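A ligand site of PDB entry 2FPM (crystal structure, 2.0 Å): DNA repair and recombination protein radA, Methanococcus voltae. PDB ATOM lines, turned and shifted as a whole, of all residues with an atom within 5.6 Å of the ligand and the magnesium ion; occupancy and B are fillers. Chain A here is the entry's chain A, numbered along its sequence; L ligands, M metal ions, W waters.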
ATOM      1  N   GLY A 105       6.130 -11.991  23.869  1.00  0.00           N
ATOM      2  CA  GLY A 105       6.768 -11.974  22.570  1.00  0.00           C
ATOM      3  C   GLY A 105       6.294 -13.083  21.670  1.00  0.00           C
ATOM      4  O   GLY A 105       5.676 -14.049  22.099  1.00  0.00           O
ATOM      5  N   VAL A 106       6.590 -12.905  20.385  1.00  0.00           N
ATOM      6  CA  VAL A 106       6.235 -13.863  19.351  1.00  0.00           C
ATOM      7  C   VAL A 106       6.890 -15.212  19.642  1.00  0.00           C
ATOM      8  O   VAL A 106       7.871 -15.296  20.390  1.00  0.00           O
ATOM      9  CB  VAL A 106       6.698 -13.316  17.972  1.00  0.00           C
ATOM     10  CG1 VAL A 106       8.199 -13.072  17.997  1.00  0.00           C
ATOM     11  CG2 VAL A 106       6.335 -14.277  16.874  1.00  0.00           C
ATOM     12  N   PHE A 107       6.335 -16.261  19.052  1.00  0.00           N
ATOM     13  CA  PHE A 107       6.853 -17.615  19.235  1.00  0.00           C
ATOM     14  C   PHE A 107       8.350 -17.625  18.943  1.00  0.00           C
ATOM     15  O   PHE A 107       8.834 -16.885  18.089  1.00  0.00           O
ATOM     16  CB  PHE A 107       6.139 -18.575  18.284  1.00  0.00           C
ATOM     17  CG  PHE A 107       6.666 -18.530  16.864  1.00  0.00           C
ATOM     18  CD1 PHE A 107       7.749 -19.318  16.477  1.00  0.00           C
ATOM     19  CD2 PHE A 107       6.118 -17.648  15.936  1.00  0.00           C
ATOM     20  CE1 PHE A 107       8.282 -19.228  15.187  1.00  0.00           C
ATOM     21  CE2 PHE A 107       6.642 -17.550  14.638  1.00  0.00           C
ATOM     22  CZ  PHE A 107       7.728 -18.334  14.265  1.00  0.00           C
ATOM     23  N   GLY A 108       9.092 -18.476  19.657  1.00  0.00           N
ATOM     24  CA  GLY A 108      10.519 -18.592  19.441  1.00  0.00           C
ATOM     25  C   GLY A 108      11.389 -17.403  19.833  1.00  0.00           C
ATOM     26  O   GLY A 108      12.601 -17.460  19.617  1.00  0.00           O
ATOM     27  N   SER A 109      10.793 -16.347  20.398  1.00  0.00           N
ATOM     28  CA  SER A 109      11.585 -15.187  20.792  1.00  0.00           C
ATOM     29  C   SER A 109      12.516 -15.471  21.971  1.00  0.00           C
ATOM     30  O   SER A 109      13.453 -14.710  22.231  1.00  0.00           O
ATOM     31  CB  SER A 109      10.663 -13.989  21.098  1.00  0.00           C
ATOM     32  OG  SER A 109       9.695 -14.284  22.081  1.00  0.00           O
ATOM     33  N   GLY A 110      12.258 -16.572  22.679  1.00  0.00           N
ATOM     34  CA  GLY A 110      13.128 -16.946  23.795  1.00  0.00           C
ATOM     35  C   GLY A 110      12.559 -16.845  25.195  1.00  0.00           C
ATOM     36  O   GLY A 110      13.300 -16.961  26.175  1.00  0.00           O
ATOM     37  N   LYS A 111      11.254 -16.623  25.308  1.00  0.00           N
ATOM     38  CA  LYS A 111      10.609 -16.508  26.611  1.00  0.00           C
ATOM     39  C   LYS A 111      10.949 -17.705  27.505  1.00  0.00           C
ATOM     40  O   LYS A 111      11.419 -17.545  28.637  1.00  0.00           O
ATOM     41  CB  LYS A 111       9.098 -16.406  26.419  1.00  0.00           C
ATOM     42  CG  LYS A 111       8.679 -15.276  25.483  1.00  0.00           C
ATOM     43  CD  LYS A 111       7.157 -15.145  25.399  1.00  0.00           C
ATOM     44  CE  LYS A 111       6.546 -16.365  24.746  1.00  0.00           C
ATOM     45  NZ  LYS A 111       6.960 -16.437  23.317  1.00  0.00           N
ATOM     46  N   THR A 112      10.741 -18.909  26.986  1.00  0.00           N
ATOM     47  CA  THR A 112      11.007 -20.118  27.752  1.00  0.00           C
ATOM     48  C   THR A 112      12.505 -20.270  28.061  1.00  0.00           C
ATOM     49  O   THR A 112      12.867 -20.779  29.123  1.00  0.00           O
ATOM     50  CB  THR A 112      10.464 -21.357  27.014  1.00  0.00           C
ATOM     51  OG1 THR A 112       9.033 -21.302  27.021  1.00  0.00           O
ATOM     52  CG2 THR A 112      10.918 -22.654  27.696  1.00  0.00           C
ATOM     53  N   GLN A 113      13.364 -19.820  27.145  1.00  0.00           N
ATOM     54  CA  GLN A 113      14.814 -19.892  27.367  1.00  0.00           C
ATOM     55  C   GLN A 113      15.181 -19.033  28.574  1.00  0.00           C
ATOM     56  O   GLN A 113      15.948 -19.444  29.440  1.00  0.00           O
ATOM     57  CB  GLN A 113      15.595 -19.385  26.145  1.00  0.00           C
ATOM     58  CG  GLN A 113      15.352 -20.173  24.864  1.00  0.00           C
ATOM     59  CD  GLN A 113      15.579 -21.659  25.046  1.00  0.00           C
ATOM     60  OE1 GLN A 113      16.708 -22.086  25.298  1.00  0.00           O
ATOM     61  NE2 GLN A 113      14.518 -22.449  24.925  1.00  0.00           N
ATOM     62  N   ILE A 114      14.625 -17.824  28.624  1.00  0.00           N
ATOM     63  CA  ILE A 114      14.899 -16.912  29.730  1.00  0.00           C
ATOM     64  C   ILE A 114      14.480 -17.534  31.063  1.00  0.00           C
ATOM     65  O   ILE A 114      15.178 -17.392  32.080  1.00  0.00           O
ATOM     66  CB  ILE A 114      14.184 -15.564  29.520  1.00  0.00           C
ATOM     67  CG1 ILE A 114      14.822 -14.830  28.335  1.00  0.00           C
ATOM     68  CG2 ILE A 114      14.278 -14.715  30.771  1.00  0.00           C
ATOM     69  CD1 ILE A 114      14.009 -13.639  27.833  1.00  0.00           C
ATOM     70  N   GLU A 151       2.610 -25.225  29.500  1.00  0.00           N
ATOM     71  CA  GLU A 151       2.535 -25.745  28.138  1.00  0.00           C
ATOM     72  C   GLU A 151       3.264 -27.057  27.878  1.00  0.00           C
ATOM     73  O   GLU A 151       3.133 -27.640  26.809  1.00  0.00           O
ATOM     74  CB  GLU A 151       3.052 -24.676  27.169  1.00  0.00           C
ATOM     75  CG  GLU A 151       2.380 -23.317  27.376  1.00  0.00           C
ATOM     76  CD  GLU A 151       2.800 -22.276  26.362  1.00  0.00           C
ATOM     77  OE1 GLU A 151       3.974 -21.864  26.374  1.00  0.00           O
ATOM     78  OE2 GLU A 151       1.959 -21.852  25.554  1.00  0.00           O
ATOM     79  N   THR A 153       6.633 -27.362  28.017  1.00  0.00           N
ATOM     80  CA  THR A 153       7.916 -27.099  27.391  1.00  0.00           C
ATOM     81  C   THR A 153       9.119 -27.051  28.333  1.00  0.00           C
ATOM     82  O   THR A 153      10.194 -26.579  27.955  1.00  0.00           O
ATOM     83  CB  THR A 153       7.877 -25.785  26.565  1.00  0.00           C
ATOM     84  OG1 THR A 153       7.210 -24.775  27.305  1.00  0.00           O
ATOM     85  CG2 THR A 153       7.147 -26.029  25.244  1.00  0.00           C
ATOM     86  N   ARG A 158      17.881 -28.884  28.694  1.00  0.00           N
ATOM     87  CA  ARG A 158      18.278 -27.492  28.477  1.00  0.00           C
ATOM     88  C   ARG A 158      18.870 -26.911  29.766  1.00  0.00           C
ATOM     89  O   ARG A 158      19.829 -26.142  29.730  1.00  0.00           O
ATOM     90  CB  ARG A 158      17.054 -26.673  28.023  1.00  0.00           C
ATOM     91  CG  ARG A 158      17.385 -25.293  27.505  1.00  0.00           C
ATOM     92  CD  ARG A 158      18.402 -25.338  26.369  1.00  0.00           C
ATOM     93  NE  ARG A 158      18.562 -24.014  25.762  1.00  0.00           N
ATOM     94  CZ  ARG A 158      19.693 -23.567  25.220  1.00  0.00           C
ATOM     95  NH1 ARG A 158      19.727 -22.341  24.700  1.00  0.00           N
ATOM     96  NH2 ARG A 158      20.776 -24.327  25.198  1.00  0.00           N
ATOM     97  N   GLN A 161      22.392 -28.392  30.038  1.00  0.00           N
ATOM     98  CA  GLN A 161      23.269 -27.756  29.064  1.00  0.00           C
ATOM     99  C   GLN A 161      23.628 -26.327  29.448  1.00  0.00           C
ATOM    100  O   GLN A 161      24.780 -25.919  29.340  1.00  0.00           O
ATOM    101  CB  GLN A 161      22.595 -27.789  27.692  1.00  0.00           C
ATOM    102  CG  GLN A 161      23.369 -27.141  26.569  1.00  0.00           C
ATOM    103  CD  GLN A 161      22.609 -27.212  25.255  1.00  0.00           C
ATOM    104  OE1 GLN A 161      21.433 -26.858  25.184  1.00  0.00           O
ATOM    105  NE2 GLN A 161      23.284 -27.676  24.204  1.00  0.00           N
ATOM    106  N   ASP A 211       5.205 -20.135  33.141  1.00  0.00           N
ATOM    107  CA  ASP A 211       5.393 -20.232  31.703  1.00  0.00           C
ATOM    108  C   ASP A 211       4.418 -21.292  31.182  1.00  0.00           C
ATOM    109  O   ASP A 211       4.684 -22.490  31.353  1.00  0.00           O
ATOM    110  CB  ASP A 211       6.842 -20.660  31.444  1.00  0.00           C
ATOM    111  CG  ASP A 211       7.197 -20.767  29.970  1.00  0.00           C
ATOM    112  OD1 ASP A 211       6.608 -20.056  29.132  1.00  0.00           O
ATOM    113  OD2 ASP A 211       8.122 -21.568  29.652  1.00  0.00           O
ATOM    114  N   GLN A 257       1.975 -14.518  25.705  1.00  0.00           N
ATOM    115  CA  GLN A 257       1.899 -14.634  24.258  1.00  0.00           C
ATOM    116  C   GLN A 257       1.405 -13.310  23.691  1.00  0.00           C
ATOM    117  O   GLN A 257       1.022 -12.413  24.433  1.00  0.00           O
ATOM    118  CB  GLN A 257       0.977 -15.791  23.901  1.00  0.00           C
ATOM    119  CG  GLN A 257       1.303 -17.045  24.722  1.00  0.00           C
ATOM    120  CD  GLN A 257       0.640 -18.305  24.209  1.00  0.00           C
ATOM    121  OE1 GLN A 257      -0.483 -18.268  23.675  1.00  0.00           O
ATOM    122  NE2 GLN A 257       1.305 -19.440  24.386  1.00  0.00           N
ATOM    123  N   ARG A 296      18.429 -11.588  19.508  1.00  0.00           N
ATOM    124  CA  ARG A 296      17.116 -11.269  20.092  1.00  0.00           C
ATOM    125  C   ARG A 296      17.158  -9.856  20.671  1.00  0.00           C
ATOM    126  O   ARG A 296      18.226  -9.325  20.994  1.00  0.00           O
ATOM    127  CB  ARG A 296      16.771 -12.259  21.219  1.00  0.00           C
ATOM    128  CG  ARG A 296      16.639 -13.712  20.802  1.00  0.00           C
ATOM    129  CD  ARG A 296      15.445 -13.944  19.911  1.00  0.00           C
ATOM    130  NE  ARG A 296      15.260 -15.354  19.586  1.00  0.00           N
ATOM    131  CZ  ARG A 296      15.929 -16.015  18.638  1.00  0.00           C
ATOM    132  NH1 ARG A 296      16.833 -15.384  17.896  1.00  0.00           N
ATOM    133  NH2 ARG A 296      15.697 -17.303  18.447  1.00  0.00           N
ATOM    134  N   ILE A 315      20.676 -16.262  21.790  1.00  0.00           N
ATOM    135  CA  ILE A 315      20.282 -17.518  22.407  1.00  0.00           C
ATOM    136  C   ILE A 315      21.123 -18.573  21.711  1.00  0.00           C
ATOM    137  O   ILE A 315      20.994 -18.783  20.503  1.00  0.00           O
ATOM    138  CB  ILE A 315      18.796 -17.860  22.178  1.00  0.00           C
ATOM    139  CG1 ILE A 315      17.894 -16.711  22.646  1.00  0.00           C
ATOM    140  CG2 ILE A 315      18.457 -19.146  22.929  1.00  0.00           C
ATOM    141  CD1 ILE A 315      18.013 -16.403  24.109  1.00  0.00           C
ATOM    142  N   THR A 316      22.013 -19.218  22.457  1.00  0.00           N
ATOM    143  CA  THR A 316      22.894 -20.227  21.875  1.00  0.00           C
ATOM    144  C   THR A 316      22.852 -21.508  22.706  1.00  0.00           C
ATOM    145  O   THR A 316      22.037 -21.638  23.610  1.00  0.00           O
ATOM    146  CB  THR A 316      24.348 -19.719  21.862  1.00  0.00           C
ATOM    147  OG1 THR A 316      24.815 -19.600  23.211  1.00  0.00           O
ATOM    148  CG2 THR A 316      24.422 -18.355  21.185  1.00  0.00           C
ATOM    149  N   GLU A 317      23.746 -22.441  22.408  1.00  0.00           N
ATOM    150  CA  GLU A 317      23.778 -23.688  23.162  1.00  0.00           C
ATOM    151  C   GLU A 317      24.099 -23.401  24.613  1.00  0.00           C
ATOM    152  O   GLU A 317      23.772 -24.190  25.501  1.00  0.00           O
ATOM    153  CB  GLU A 317      24.817 -24.669  22.582  1.00  0.00           C
ATOM    154  CG  GLU A 317      25.663 -24.143  21.423  1.00  0.00           C
ATOM    155  CD  GLU A 317      26.709 -23.132  21.864  1.00  0.00           C
ATOM    156  OE1 GLU A 317      27.595 -23.503  22.657  1.00  0.00           O
ATOM    157  OE2 GLU A 317      26.643 -21.979  21.397  1.00  0.00           O
HETATM  158  P1  LIG L   1       6.782 -20.066  22.506  1.00  0.00           P
HETATM  159  O1  LIG L   1       6.596 -20.616  23.822  1.00  0.00           O
HETATM  160  O2  LIG L   1       6.257 -21.017  21.495  1.00  0.00           O
HETATM  161  O3  LIG L   1       6.076 -18.805  22.371  1.00  0.00           O
HETATM  162  P2  LIG L   1       9.413 -19.145  23.208  1.00  0.00           P
HETATM  163  O4  LIG L   1       9.231 -19.686  24.573  1.00  0.00           O
HETATM  164  O5  LIG L   1       9.244 -17.692  23.198  1.00  0.00           O
HETATM  165  N1  LIG L   1       8.412 -19.820  22.196  1.00  0.00           N
HETATM  166  P3  LIG L   1      11.828 -20.623  23.246  1.00  0.00           P
HETATM  167  O6  LIG L   1      12.221 -20.330  24.694  1.00  0.00           O
HETATM  168  O7  LIG L   1      11.119 -21.921  23.159  1.00  0.00           O
HETATM  169  O8  LIG L   1      10.898 -19.426  22.680  1.00  0.00           O
HETATM  170  O9  LIG L   1      13.200 -20.643  22.318  1.00  0.00           O
HETATM  171  C1  LIG L   1      13.233 -21.297  20.945  1.00  0.00           C
HETATM  172  C2  LIG L   1      14.422 -21.052  20.382  1.00  0.00           C
HETATM  173  O10 LIG L   1      15.495 -21.305  21.374  1.00  0.00           O
HETATM  174  C3  LIG L   1      14.732 -22.125  19.293  1.00  0.00           C
HETATM  175  O11 LIG L   1      13.915 -22.122  18.184  1.00  0.00           O
HETATM  176  C4  LIG L   1      16.275 -22.203  19.265  1.00  0.00           C
HETATM  177  O12 LIG L   1      16.779 -21.177  18.234  1.00  0.00           O
HETATM  178  C5  LIG L   1      16.694 -21.713  20.657  1.00  0.00           C
HETATM  179  N2  LIG L   1      17.246 -22.790  21.255  1.00  0.00           N
HETATM  180  C6  LIG L   1      16.618 -23.720  22.101  1.00  0.00           C
HETATM  181  N3  LIG L   1      17.471 -24.618  22.451  1.00  0.00           N
HETATM  182  C7  LIG L   1      18.666 -24.343  21.887  1.00  0.00           C
HETATM  183  C8  LIG L   1      19.903 -24.955  21.909  1.00  0.00           C
HETATM  184  N4  LIG L   1      20.087 -26.090  22.627  1.00  0.00           N
HETATM  185  N5  LIG L   1      20.968 -24.387  21.180  1.00  0.00           N
HETATM  186  C9  LIG L   1      20.785 -23.198  20.421  1.00  0.00           C
HETATM  187  N6  LIG L   1      19.575 -22.569  20.367  1.00  0.00           N
HETATM  188  C10 LIG L   1      18.537 -23.189  21.131  1.00  0.00           C
HETATM  189 MG    MG M   1       7.866 -20.959  25.365  1.00  0.00          MG
HETATM  190  O   HOH W   1       8.789 -22.613  24.377  1.00  0.00           O
HETATM  191  O   HOH W   2       4.323 -19.457  25.219  1.00  0.00           O
HETATM  192  O   HOH W   3       6.745 -19.504  26.656  1.00  0.00           O
HETATM  193  O   HOH W   4      15.242 -20.667  16.205  1.00  0.00           O
HETATM  194  O   HOH W   5       6.984 -23.560  22.690  1.00  0.00           O
HETATM  195  O   HOH W   6       6.479 -22.371  26.030  1.00  0.00           O
HETATM  196  O   HOH W   7      22.449 -27.881  21.410  1.00  0.00           O
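The backbone NH of Gly 108 sits close to a nitrogen (N1) of the ligand, at 3.0 Å. NH2 of Arg 158 lies close to N4 of the ligand. Residues that only touch the ligand: Phe 107 (3.4 Å), Glu 317 (3.5 Å), Thr 316 (3.5 Å), Ile 315 (3.9 Å), Glu 151 (3.9 Å) and Val 106 (3.9 Å). Hydrophobic or aromatic side chains that line the ligand: Ile 315.
Water W6 lies within hydrogen-bond range of OE1 of Glu 151 (2.6 Å) and OG1 of Thr 153 (2.8 Å). Water W2 lies within hydrogen-bond range of the side-chain carboxylate of Glu 151 (2.7 Å), the side-chain amide nitrogen of Gln 257 (3.1 Å) and an oxygen (O3) of the ligand (3.4 Å). Water W7 bridges NE2 of Gln 161 (2.9 Å) and N4 of the ligand (3.2 Å).
N of Thr 112 is in hydrogen-bond range of O6 of the ligand, 3.1 Å away. N of Lys 111 is in hydrogen-bond range of O5 of the ligand (3.1 Å). O5 of the ligand is in salt-bridge range of NZ of Lys 111. O6 of the ligand lies within hydrogen-bond range of N of Gln 113. An oxygen (O6) of the ligand sits at hydrogen-bond distance from the side-chain amide nitrogen (NE2) of Gln 113, at 3.1 Å. A nitrogen (N4) of the ligand sits at hydrogen-bond distance from the side-chain amide oxygen (OE1) of Gln 161 (3.0 Å). The backbone NH (N) of Gly 110 sits at hydrogen-bond distance from an oxygen (O8) of the ligand, at 3.2 Å. N of Ser 109 lies within hydrogen-bond range of O5 of the ligand (3.5 Å).
The magnesium ion is bound by an oxygen (O4) of the ligand (2.0 Å), an oxygen (O1) of the ligand (2.0 Å), the side-chain hydroxyl of Thr 112 (2.1 Å), water W6 (2.1 Å), water W1 (2.1 Å) and water W3 (2.2 Å).
The side-chain amino group (NZ) of Lys 111 sits at hydrogen-bond distance from the backbone carbonyl oxygen (O) of Gly 105. OE1 of Gln 113 is in hydrogen-bond range of NE of Arg 158 (2.7 Å). The backbone carbonyl oxygen (O) of Gly 108 is in hydrogen-bond range of the guanidinium group (NH2) of Arg 296, at 3.3 Å. The side-chain amide oxygen (OE1) of Gln 161 is in hydrogen-bond range of the guanidinium group (NH2) of Arg 158 (2.6 Å). The guanidinium group (NH2) of Arg 158 lies within hydrogen-bond range of the backbone carbonyl oxygen (O) of Glu 317. O of Thr 316 sits at hydrogen-bond distance from NH1 of Arg 158, 2.6 Å away. O of Ser 109 lies close to NE of Arg 296. The side-chain carboxylate of Glu 151 sits at hydrogen-bond distance from the side-chain amide nitrogen of Gln 257 (2.8 Å).
Within 4 Å of the magnesium ion: Thr 112. The nearest printed residue that does not touch the magnesium ion is Asp 211 (4.1 Å).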
